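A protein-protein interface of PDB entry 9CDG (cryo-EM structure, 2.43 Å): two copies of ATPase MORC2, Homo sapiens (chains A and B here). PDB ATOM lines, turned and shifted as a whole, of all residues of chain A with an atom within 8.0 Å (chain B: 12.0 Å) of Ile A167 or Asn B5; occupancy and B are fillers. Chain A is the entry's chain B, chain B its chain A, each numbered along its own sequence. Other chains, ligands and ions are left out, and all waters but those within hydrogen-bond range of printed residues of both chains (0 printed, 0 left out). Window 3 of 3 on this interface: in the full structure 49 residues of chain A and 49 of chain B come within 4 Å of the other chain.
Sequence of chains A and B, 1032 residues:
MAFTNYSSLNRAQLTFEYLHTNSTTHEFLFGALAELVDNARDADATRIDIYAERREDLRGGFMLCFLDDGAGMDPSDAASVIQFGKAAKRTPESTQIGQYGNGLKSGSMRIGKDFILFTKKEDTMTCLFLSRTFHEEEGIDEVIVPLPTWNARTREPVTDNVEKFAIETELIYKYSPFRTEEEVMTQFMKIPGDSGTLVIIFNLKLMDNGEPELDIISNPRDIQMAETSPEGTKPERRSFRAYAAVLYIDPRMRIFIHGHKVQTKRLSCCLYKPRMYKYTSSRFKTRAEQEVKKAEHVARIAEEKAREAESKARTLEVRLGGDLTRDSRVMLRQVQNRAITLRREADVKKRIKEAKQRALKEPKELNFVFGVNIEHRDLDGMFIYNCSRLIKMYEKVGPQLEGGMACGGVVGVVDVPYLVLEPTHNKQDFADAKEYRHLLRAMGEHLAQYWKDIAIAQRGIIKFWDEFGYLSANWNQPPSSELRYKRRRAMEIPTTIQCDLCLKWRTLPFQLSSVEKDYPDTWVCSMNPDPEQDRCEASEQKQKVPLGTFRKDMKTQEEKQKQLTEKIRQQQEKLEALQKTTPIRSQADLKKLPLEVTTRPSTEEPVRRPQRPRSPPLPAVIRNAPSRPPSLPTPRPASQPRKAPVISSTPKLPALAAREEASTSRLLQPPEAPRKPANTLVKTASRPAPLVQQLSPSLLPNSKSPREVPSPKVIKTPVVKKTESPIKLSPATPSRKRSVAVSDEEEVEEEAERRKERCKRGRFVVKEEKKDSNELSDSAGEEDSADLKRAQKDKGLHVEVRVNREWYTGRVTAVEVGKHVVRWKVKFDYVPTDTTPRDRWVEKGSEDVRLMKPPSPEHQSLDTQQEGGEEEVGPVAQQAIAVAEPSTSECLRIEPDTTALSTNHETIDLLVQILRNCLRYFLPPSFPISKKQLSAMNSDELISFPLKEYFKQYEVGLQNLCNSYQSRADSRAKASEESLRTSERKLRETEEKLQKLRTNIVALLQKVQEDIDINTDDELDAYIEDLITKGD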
ATOM      1  N   PHE A 134     -24.310  22.981 -19.381  1.00  0.00           N
ATOM      2  CA  PHE A 134     -24.144  22.004 -18.312  1.00  0.00           C
ATOM      3  C   PHE A 134     -24.783  20.673 -18.684  1.00  0.00           C
ATOM      4  O   PHE A 134     -24.196  19.611 -18.445  1.00  0.00           O
ATOM      5  CB  PHE A 134     -24.728  22.568 -17.012  1.00  0.00           C
ATOM      6  CG  PHE A 134     -25.192  21.527 -16.026  1.00  0.00           C
ATOM      7  CD1 PHE A 134     -24.293  20.670 -15.404  1.00  0.00           C
ATOM      8  CD2 PHE A 134     -26.529  21.446 -15.682  1.00  0.00           C
ATOM      9  CE1 PHE A 134     -24.731  19.728 -14.492  1.00  0.00           C
ATOM     10  CE2 PHE A 134     -26.970  20.512 -14.767  1.00  0.00           C
ATOM     11  CZ  PHE A 134     -26.068  19.653 -14.172  1.00  0.00           C
ATOM     12  N   GLU A 138     -22.538  17.316 -19.186  1.00  0.00           N
ATOM     13  CA  GLU A 138     -22.714  16.254 -18.214  1.00  0.00           C
ATOM     14  C   GLU A 138     -23.667  15.159 -18.661  1.00  0.00           C
ATOM     15  O   GLU A 138     -23.786  14.151 -17.954  1.00  0.00           O
ATOM     16  CB  GLU A 138     -23.196  16.832 -16.877  1.00  0.00           C
ATOM     17  CG  GLU A 138     -22.195  17.778 -16.258  1.00  0.00           C
ATOM     18  CD  GLU A 138     -21.912  17.452 -14.813  1.00  0.00           C
ATOM     19  OE1 GLU A 138     -22.076  16.277 -14.423  1.00  0.00           O
ATOM     20  OE2 GLU A 138     -21.520  18.369 -14.063  1.00  0.00           O
ATOM     21  N   ILE A 144     -32.097  20.562 -14.913  1.00  0.00           N
ATOM     22  CA  ILE A 144     -31.575  20.811 -13.576  1.00  0.00           C
ATOM     23  C   ILE A 144     -31.146  22.270 -13.500  1.00  0.00           C
ATOM     24  O   ILE A 144     -30.278  22.713 -14.262  1.00  0.00           O
ATOM     25  CB  ILE A 144     -30.412  19.862 -13.251  1.00  0.00           C
ATOM     26  CG1 ILE A 144     -30.942  18.451 -13.009  1.00  0.00           C
ATOM     27  CG2 ILE A 144     -29.639  20.348 -12.053  1.00  0.00           C
ATOM     28  CD1 ILE A 144     -29.881  17.461 -12.602  1.00  0.00           C
ATOM     29  N   PRO A 146     -29.718  25.176 -10.980  1.00  0.00           N
ATOM     30  CA  PRO A 146     -29.223  25.735  -9.716  1.00  0.00           C
ATOM     31  C   PRO A 146     -29.957  27.006  -9.319  1.00  0.00           C
ATOM     32  O   PRO A 146     -30.091  27.942 -10.109  1.00  0.00           O
ATOM     33  CB  PRO A 146     -27.747  26.003 -10.011  1.00  0.00           C
ATOM     34  CG  PRO A 146     -27.391  24.951 -10.984  1.00  0.00           C
ATOM     35  CD  PRO A 146     -28.611  24.723 -11.838  1.00  0.00           C
ATOM     36  N   LEU A 147     -30.441  27.026  -8.079  1.00  0.00           N
ATOM     37  CA  LEU A 147     -31.136  28.182  -7.515  1.00  0.00           C
ATOM     38  C   LEU A 147     -30.617  28.501  -6.118  1.00  0.00           C
ATOM     39  O   LEU A 147     -31.282  28.199  -5.119  1.00  0.00           O
ATOM     40  CB  LEU A 147     -32.643  27.937  -7.473  1.00  0.00           C
ATOM     41  CG  LEU A 147     -33.413  28.476  -8.670  1.00  0.00           C
ATOM     42  CD1 LEU A 147     -34.742  27.765  -8.809  1.00  0.00           C
ATOM     43  CD2 LEU A 147     -33.607  29.955  -8.494  1.00  0.00           C
ATOM     44  N   PRO A 148     -29.441  29.116  -6.003  1.00  0.00           N
ATOM     45  CA  PRO A 148     -28.966  29.522  -4.682  1.00  0.00           C
ATOM     46  C   PRO A 148     -29.480  30.897  -4.291  1.00  0.00           C
ATOM     47  O   PRO A 148     -29.813  31.732  -5.133  1.00  0.00           O
ATOM     48  CB  PRO A 148     -27.446  29.531  -4.854  1.00  0.00           C
ATOM     49  CG  PRO A 148     -27.257  29.917  -6.237  1.00  0.00           C
ATOM     50  CD  PRO A 148     -28.408  29.361  -7.026  1.00  0.00           C
ATOM     51  N   ASN A 161     -30.033  23.478   2.842  1.00  0.00           N
ATOM     52  CA  ASN A 161     -29.259  22.330   2.379  1.00  0.00           C
ATOM     53  C   ASN A 161     -27.907  22.857   1.903  1.00  0.00           C
ATOM     54  O   ASN A 161     -27.791  23.346   0.775  1.00  0.00           O
ATOM     55  CB  ASN A 161     -30.007  21.596   1.277  1.00  0.00           C
ATOM     56  CG  ASN A 161     -29.617  20.143   1.176  1.00  0.00           C
ATOM     57  OD1 ASN A 161     -28.441  19.801   1.235  1.00  0.00           O
ATOM     58  ND2 ASN A 161     -30.607  19.274   1.021  1.00  0.00           N
ATOM     59  N   VAL A 162     -26.900  22.751   2.771  1.00  0.00           N
ATOM     60  CA  VAL A 162     -25.602  23.363   2.504  1.00  0.00           C
ATOM     61  C   VAL A 162     -24.849  22.650   1.386  1.00  0.00           C
ATOM     62  O   VAL A 162     -24.180  23.306   0.578  1.00  0.00           O
ATOM     63  CB  VAL A 162     -24.766  23.422   3.794  1.00  0.00           C
ATOM     64  CG1 VAL A 162     -25.162  24.633   4.617  1.00  0.00           C
ATOM     65  CG2 VAL A 162     -24.952  22.158   4.609  1.00  0.00           C
ATOM     66  N   GLU A 163     -24.932  21.318   1.308  1.00  0.00           N
ATOM     67  CA  GLU A 163     -24.267  20.619   0.213  1.00  0.00           C
ATOM     68  C   GLU A 163     -24.966  20.877  -1.114  1.00  0.00           C
ATOM     69  O   GLU A 163     -24.302  20.944  -2.154  1.00  0.00           O
ATOM     70  CB  GLU A 163     -24.185  19.115   0.488  1.00  0.00           C
ATOM     71  CG  GLU A 163     -25.474  18.466   0.954  1.00  0.00           C
ATOM     72  CD  GLU A 163     -25.584  18.374   2.463  1.00  0.00           C
ATOM     73  OE1 GLU A 163     -24.918  19.165   3.160  1.00  0.00           O
ATOM     74  OE2 GLU A 163     -26.343  17.513   2.953  1.00  0.00           O
ATOM     75  N   LYS A 164     -26.291  21.048  -1.094  1.00  0.00           N
ATOM     76  CA  LYS A 164     -27.012  21.447  -2.299  1.00  0.00           C
ATOM     77  C   LYS A 164     -26.602  22.845  -2.743  1.00  0.00           C
ATOM     78  O   LYS A 164     -26.430  23.090  -3.943  1.00  0.00           O
ATOM     79  CB  LYS A 164     -28.518  21.378  -2.057  1.00  0.00           C
ATOM     80  CG  LYS A 164     -29.371  21.973  -3.164  1.00  0.00           C
ATOM     81  CD  LYS A 164     -30.765  22.293  -2.673  1.00  0.00           C
ATOM     82  CE  LYS A 164     -31.577  22.977  -3.754  1.00  0.00           C
ATOM     83  NZ  LYS A 164     -33.028  22.971  -3.434  1.00  0.00           N
ATOM     84  N   PHE A 165     -26.427  23.765  -1.785  1.00  0.00           N
ATOM     85  CA  PHE A 165     -25.925  25.100  -2.103  1.00  0.00           C
ATOM     86  C   PHE A 165     -24.529  25.038  -2.705  1.00  0.00           C
ATOM     87  O   PHE A 165     -24.226  25.763  -3.658  1.00  0.00           O
ATOM     88  CB  PHE A 165     -25.913  25.977  -0.848  1.00  0.00           C
ATOM     89  CG  PHE A 165     -25.380  27.371  -1.081  1.00  0.00           C
ATOM     90  CD1 PHE A 165     -26.205  28.366  -1.574  1.00  0.00           C
ATOM     91  CD2 PHE A 165     -24.053  27.686  -0.807  1.00  0.00           C
ATOM     92  CE1 PHE A 165     -25.720  29.641  -1.788  1.00  0.00           C
ATOM     93  CE2 PHE A 165     -23.563  28.949  -1.045  1.00  0.00           C
ATOM     94  CZ  PHE A 165     -24.401  29.931  -1.526  1.00  0.00           C
ATOM     95  N   ALA A 166     -23.660  24.198  -2.134  1.00  0.00           N
ATOM     96  CA  ALA A 166     -22.302  24.051  -2.644  1.00  0.00           C
ATOM     97  C   ALA A 166     -22.291  23.486  -4.057  1.00  0.00           C
ATOM     98  O   ALA A 166     -21.528  23.963  -4.902  1.00  0.00           O
ATOM     99  CB  ALA A 166     -21.485  23.158  -1.713  1.00  0.00           C
ATOM    100  N   ILE A 167     -23.150  22.500  -4.328  1.00  0.00           N
ATOM    101  CA  ILE A 167     -23.254  21.921  -5.663  1.00  0.00           C
ATOM    102  C   ILE A 167     -23.778  22.950  -6.663  1.00  0.00           C
ATOM    103  O   ILE A 167     -23.232  23.088  -7.768  1.00  0.00           O
ATOM    104  CB  ILE A 167     -24.135  20.659  -5.612  1.00  0.00           C
ATOM    105  CG1 ILE A 167     -23.379  19.513  -4.943  1.00  0.00           C
ATOM    106  CG2 ILE A 167     -24.561  20.234  -6.987  1.00  0.00           C
ATOM    107  CD1 ILE A 167     -24.274  18.408  -4.445  1.00  0.00           C
ATOM    108  N   GLU A 168     -24.811  23.712  -6.277  1.00  0.00           N
ATOM    109  CA  GLU A 168     -25.375  24.743  -7.148  1.00  0.00           C
ATOM    110  C   GLU A 168     -24.361  25.833  -7.459  1.00  0.00           C
ATOM    111  O   GLU A 168     -24.213  26.240  -8.617  1.00  0.00           O
ATOM    112  CB  GLU A 168     -26.605  25.372  -6.495  1.00  0.00           C
ATOM    113  CG  GLU A 168     -27.851  24.521  -6.499  1.00  0.00           C
ATOM    114  CD  GLU A 168     -28.938  25.100  -5.619  1.00  0.00           C
ATOM    115  OE1 GLU A 168     -28.640  25.435  -4.455  1.00  0.00           O
ATOM    116  OE2 GLU A 168     -30.087  25.221  -6.088  1.00  0.00           O
ATOM    117  N   THR A 169     -23.634  26.294  -6.440  1.00  0.00           N
ATOM    118  CA  THR A 169     -22.678  27.371  -6.646  1.00  0.00           C
ATOM    119  C   THR A 169     -21.472  26.901  -7.442  1.00  0.00           C
ATOM    120  O   THR A 169     -20.981  27.638  -8.298  1.00  0.00           O
ATOM    121  CB  THR A 169     -22.245  27.951  -5.308  1.00  0.00           C
ATOM    122  OG1 THR A 169     -22.021  26.887  -4.376  1.00  0.00           O
ATOM    123  CG2 THR A 169     -23.327  28.849  -4.776  1.00  0.00           C
ATOM    124  N   GLU A 170     -20.992  25.677  -7.190  1.00  0.00           N
ATOM    125  CA  GLU A 170     -19.893  25.131  -7.978  1.00  0.00           C
ATOM    126  C   GLU A 170     -20.298  24.925  -9.428  1.00  0.00           C
ATOM    127  O   GLU A 170     -19.485  25.138 -10.334  1.00  0.00           O
ATOM    128  CB  GLU A 170     -19.417  23.812  -7.374  1.00  0.00           C
ATOM    129  CG  GLU A 170     -18.402  23.972  -6.260  1.00  0.00           C
ATOM    130  CD  GLU A 170     -18.487  22.859  -5.236  1.00  0.00           C
ATOM    131  OE1 GLU A 170     -19.204  21.870  -5.492  1.00  0.00           O
ATOM    132  OE2 GLU A 170     -17.841  22.976  -4.174  1.00  0.00           O
ATOM    133  N   LEU A 171     -21.556  24.548  -9.661  1.00  0.00           N
ATOM    134  CA  LEU A 171     -22.069  24.425 -11.017  1.00  0.00           C
ATOM    135  C   LEU A 171     -22.130  25.783 -11.704  1.00  0.00           C
ATOM    136  O   LEU A 171     -21.823  25.891 -12.901  1.00  0.00           O
ATOM    137  CB  LEU A 171     -23.453  23.778 -10.963  1.00  0.00           C
ATOM    138  CG  LEU A 171     -23.898  22.890 -12.119  1.00  0.00           C
ATOM    139  CD1 LEU A 171     -24.414  23.683 -13.310  1.00  0.00           C
ATOM    140  CD2 LEU A 171     -22.734  21.987 -12.494  1.00  0.00           C
ATOM    141  N   ILE A 172     -22.517  26.817 -10.956  1.00  0.00           N
ATOM    142  CA  ILE A 172     -22.531  28.179 -11.480  1.00  0.00           C
ATOM    143  C   ILE A 172     -21.119  28.645 -11.813  1.00  0.00           C
ATOM    144  O   ILE A 172     -20.881  29.224 -12.873  1.00  0.00           O
ATOM    145  CB  ILE A 172     -23.226  29.113 -10.473  1.00  0.00           C
ATOM    146  CG1 ILE A 172     -24.727  28.869 -10.503  1.00  0.00           C
ATOM    147  CG2 ILE A 172     -22.958  30.573 -10.783  1.00  0.00           C
ATOM    148  CD1 ILE A 172     -25.454  29.540  -9.406  1.00  0.00           C
ATOM    149  N   TYR A 173     -20.154  28.365 -10.942  1.00  0.00           N
ATOM    150  CA  TYR A 173     -18.788  28.802 -11.213  1.00  0.00           C
ATOM    151  C   TYR A 173     -18.130  27.983 -12.314  1.00  0.00           C
ATOM    152  O   TYR A 173     -17.164  28.455 -12.920  1.00  0.00           O
ATOM    153  CB  TYR A 173     -17.913  28.739  -9.953  1.00  0.00           C
ATOM    154  CG  TYR A 173     -18.494  29.376  -8.706  1.00  0.00           C
ATOM    155  CD1 TYR A 173     -19.311  30.502  -8.774  1.00  0.00           C
ATOM    156  CD2 TYR A 173     -18.221  28.841  -7.454  1.00  0.00           C
ATOM    157  CE1 TYR A 173     -19.849  31.061  -7.635  1.00  0.00           C
ATOM    158  CE2 TYR A 173     -18.755  29.395  -6.312  1.00  0.00           C
ATOM    159  CZ  TYR A 173     -19.563  30.504  -6.409  1.00  0.00           C
ATOM    160  OH  TYR A 173     -20.093  31.054  -5.270  1.00  0.00           O
ATOM    161  N   LYS A 174     -18.626  26.778 -12.584  1.00  0.00           N
ATOM    162  CA  LYS A 174     -18.123  25.963 -13.679  1.00  0.00           C
ATOM    163  C   LYS A 174     -18.685  26.365 -15.035  1.00  0.00           C
ATOM    164  O   LYS A 174     -17.921  26.506 -15.994  1.00  0.00           O
ATOM    165  CB  LYS A 174     -18.432  24.486 -13.422  1.00  0.00           C
ATOM    166  CG  LYS A 174     -17.882  23.548 -14.479  1.00  0.00           C
ATOM    167  CD  LYS A 174     -17.915  22.101 -14.024  1.00  0.00           C
ATOM    168  CE  LYS A 174     -17.144  21.904 -12.734  1.00  0.00           C
ATOM    169  NZ  LYS A 174     -16.917  20.461 -12.448  1.00  0.00           N
ATOM    170  N   THR B   4     -20.957  14.679 -10.513  1.00  0.00           N
ATOM    171  CA  THR B   4     -21.396  14.092  -9.253  1.00  0.00           C
ATOM    172  C   THR B   4     -22.917  13.999  -9.191  1.00  0.00           C
ATOM    173  O   THR B   4     -23.604  14.222 -10.186  1.00  0.00           O
ATOM    174  CB  THR B   4     -20.886  14.900  -8.046  1.00  0.00           C
ATOM    175  OG1 THR B   4     -21.445  14.367  -6.839  1.00  0.00           O
ATOM    176  CG2 THR B   4     -21.275  16.362  -8.178  1.00  0.00           C
ATOM    177  N   ASN B   5     -23.435  13.668  -8.013  1.00  0.00           N
ATOM    178  CA  ASN B   5     -24.867  13.489  -7.833  1.00  0.00           C
ATOM    179  C   ASN B   5     -25.572  14.833  -7.706  1.00  0.00           C
ATOM    180  O   ASN B   5     -25.135  15.713  -6.960  1.00  0.00           O
ATOM    181  CB  ASN B   5     -25.140  12.638  -6.593  1.00  0.00           C
ATOM    182  CG  ASN B   5     -26.610  12.560  -6.255  1.00  0.00           C
ATOM    183  OD1 ASN B   5     -27.381  11.884  -6.934  1.00  0.00           O
ATOM    184  ND2 ASN B   5     -27.009  13.255  -5.196  1.00  0.00           N
ATOM    185  N   TYR B   6     -26.672  14.984  -8.442  1.00  0.00           N
ATOM    186  CA  TYR B   6     -27.494  16.186  -8.401  1.00  0.00           C
ATOM    187  C   TYR B   6     -28.921  15.870  -7.971  1.00  0.00           C
ATOM    188  O   TYR B   6     -29.866  16.512  -8.428  1.00  0.00           O
ATOM    189  CB  TYR B   6     -27.494  16.892  -9.756  1.00  0.00           C
ATOM    190  CG  TYR B   6     -26.115  17.147 -10.306  1.00  0.00           C
ATOM    191  CD1 TYR B   6     -25.174  17.825  -9.553  1.00  0.00           C
ATOM    192  CD2 TYR B   6     -25.755  16.716 -11.576  1.00  0.00           C
ATOM    193  CE1 TYR B   6     -23.910  18.069 -10.038  1.00  0.00           C
ATOM    194  CE2 TYR B   6     -24.486  16.956 -12.074  1.00  0.00           C
ATOM    195  CZ  TYR B   6     -23.569  17.633 -11.295  1.00  0.00           C
ATOM    196  OH  TYR B   6     -22.303  17.883 -11.765  1.00  0.00           O
ATOM    197  N   SER B   7     -29.086  14.874  -7.096  1.00  0.00           N
ATOM    198  CA  SER B   7     -30.419  14.449  -6.683  1.00  0.00           C
ATOM    199  C   SER B   7     -31.114  15.496  -5.824  1.00  0.00           C
ATOM    200  O   SER B   7     -32.324  15.701  -5.960  1.00  0.00           O
ATOM    201  CB  SER B   7     -30.337  13.124  -5.929  1.00  0.00           C
ATOM    202  OG  SER B   7     -29.900  13.328  -4.598  1.00  0.00           O
ATOM    203  N   SER B   8     -30.374  16.170  -4.950  1.00  0.00           N
ATOM    204  CA  SER B   8     -30.950  17.182  -4.074  1.00  0.00           C
ATOM    205  C   SER B   8     -31.178  18.512  -4.772  1.00  0.00           C
ATOM    206  O   SER B   8     -31.773  19.413  -4.174  1.00  0.00           O
ATOM    207  CB  SER B   8     -30.047  17.396  -2.859  1.00  0.00           C
ATOM    208  OG  SER B   8     -28.815  17.977  -3.244  1.00  0.00           O
ATOM    209  N   LEU B   9     -30.729  18.653  -6.010  1.00  0.00           N
ATOM    210  CA  LEU B   9     -30.777  19.918  -6.718  1.00  0.00           C
ATOM    211  C   LEU B   9     -32.154  20.094  -7.352  1.00  0.00           C
ATOM    212  O   LEU B   9     -32.809  19.120  -7.730  1.00  0.00           O
ATOM    213  CB  LEU B   9     -29.667  19.951  -7.771  1.00  0.00           C
ATOM    214  CG  LEU B   9     -28.918  21.241  -8.112  1.00  0.00           C
ATOM    215  CD1 LEU B   9     -27.678  20.907  -8.913  1.00  0.00           C
ATOM    216  CD2 LEU B   9     -29.760  22.208  -8.879  1.00  0.00           C
ATOM    217  N   ASN B  10     -32.597  21.348  -7.431  1.00  0.00           N
ATOM    218  CA  ASN B  10     -33.904  21.677  -7.987  1.00  0.00           C
ATOM    219  C   ASN B  10     -33.979  21.342  -9.472  1.00  0.00           C
ATOM    220  O   ASN B  10     -32.993  21.430 -10.206  1.00  0.00           O
ATOM    221  CB  ASN B  10     -34.206  23.161  -7.785  1.00  0.00           C
ATOM    222  CG  ASN B  10     -34.933  23.435  -6.491  1.00  0.00           C
ATOM    223  OD1 ASN B  10     -34.525  22.976  -5.425  1.00  0.00           O
ATOM    224  ND2 ASN B  10     -36.022  24.189  -6.575  1.00  0.00           N
ATOM    225  N   ARG B  11     -35.172  20.951  -9.907  1.00  0.00           N
ATOM    226  CA  ARG B  11     -35.437  20.607 -11.294  1.00  0.00           C
ATOM    227  C   ARG B  11     -36.611  21.421 -11.805  1.00  0.00           C
ATOM    228  O   ARG B  11     -37.519  21.770 -11.047  1.00  0.00           O
ATOM    229  CB  ARG B  11     -35.749  19.117 -11.463  1.00  0.00           C
ATOM    230  CG  ARG B  11     -34.572  18.288 -11.907  1.00  0.00           C
ATOM    231  CD  ARG B  11     -33.968  17.564 -10.734  1.00  0.00           C
ATOM    232  NE  ARG B  11     -33.075  16.498 -11.161  1.00  0.00           N
ATOM    233  CZ  ARG B  11     -32.239  15.865 -10.352  1.00  0.00           C
ATOM    234  NH1 ARG B  11     -32.161  16.170  -9.068  1.00  0.00           N
ATOM    235  NH2 ARG B  11     -31.459  14.908 -10.844  1.00  0.00           N
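OH of Tyr B6 sits at hydrogen-bond distance from OE2 of Glu A138, at 2.5 Å.
The side-chain amide oxygen (OD1) of Asn B10 lies within hydrogen-bond range of the side-chain amino group (NZ) of Lys A164 (2.5 Å).
OG of Ser B7 lies within hydrogen-bond range of ND2 of Asn B5, 3.0 Å away.
The backbone carbonyl oxygen of Tyr B6 is in hydrogen-bond range of the guanidinium group of Arg B11 (2.4 Å).
The backbone carbonyl oxygen (O) of Ser B7 sits at hydrogen-bond distance from the guanidinium group (NH1) of Arg B11, 3.1 Å away.
The backbone carbonyl oxygen (O) of Leu B9 sits at hydrogen-bond distance from the guanidinium group (NH1) of Arg B11 (3.3 Å).
The side-chain carboxylate of Glu A168 sits at hydrogen-bond distance from the backbone NH of Leu A147.
The backbone NH (N) of Lys A164 lies within hydrogen-bond range of the side-chain amide oxygen (OD1) of Asn A161, 3.4 Å away.
Among the printed residues, merely in contact across the chains: Phe A134 with Tyr B6, Ile A144 with Tyr B6, Ile A144 with Leu B9, Ile A144 with Asn B10, Ile A144 with Arg B11, Pro A146 with Leu B9, Lys A164 with Ser B8, Ile A167 with Asn B5, Ile A167 with Tyr B6, Ile A167 with Leu B9 and Glu A168 with Leu B9.
Of chain B, only Asn B5 (3.8 Å), Tyr B6 (3.6 Å) and Leu B9 (3.7 Å) come within 4 Å of Ile A167.
Of chain A, only Ile A167 (3.8 Å) comes within 4 Å of Asn B5.
No residue of chain B comes within 4 Å of Glu A163.
No residue of chain B comes within 4 Å of Ala A166.
No residue of chain B comes within 4 Å of Thr A169.
No residue of chain B comes within 4 Å of Glu A170.
Leu A171 touches none of the printed residues of chain B.
Thr B4 touches none of the printed residues of chain A.
Printed residues of chain B within 4 Å of Glu A138: Tyr B6.
Printed residues of chain A within 4 Å of Tyr B6: Phe A134 (3.7 Å), Glu A138 (2.5 Å), Ile A144 (3.8 Å) and Ile A167 (3.6 Å).
Printed residues of chain A within 4 Å of Asn B10: Ile A144 and Lys A164.
Asn A161 touches none of the printed residues of chain B.
The nearest printed residue of chain A that does not touch Asn B5 is Ile A144 (7.0 Å).
The nearest printed residue of chain B that does not touch Pro A146 is Asn B10 (5.0 Å).
Of the 20 printed residues of chain A, 7 touch a printed residue of chain B.
Of the 8 printed residues of chain B, 6 touch a printed residue of chain A.
Hydrophobic or aromatic side chains of chain B within 4 Å of the printed part of chain A: Tyr B6 and Leu B9.
No position is printed for both chains.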
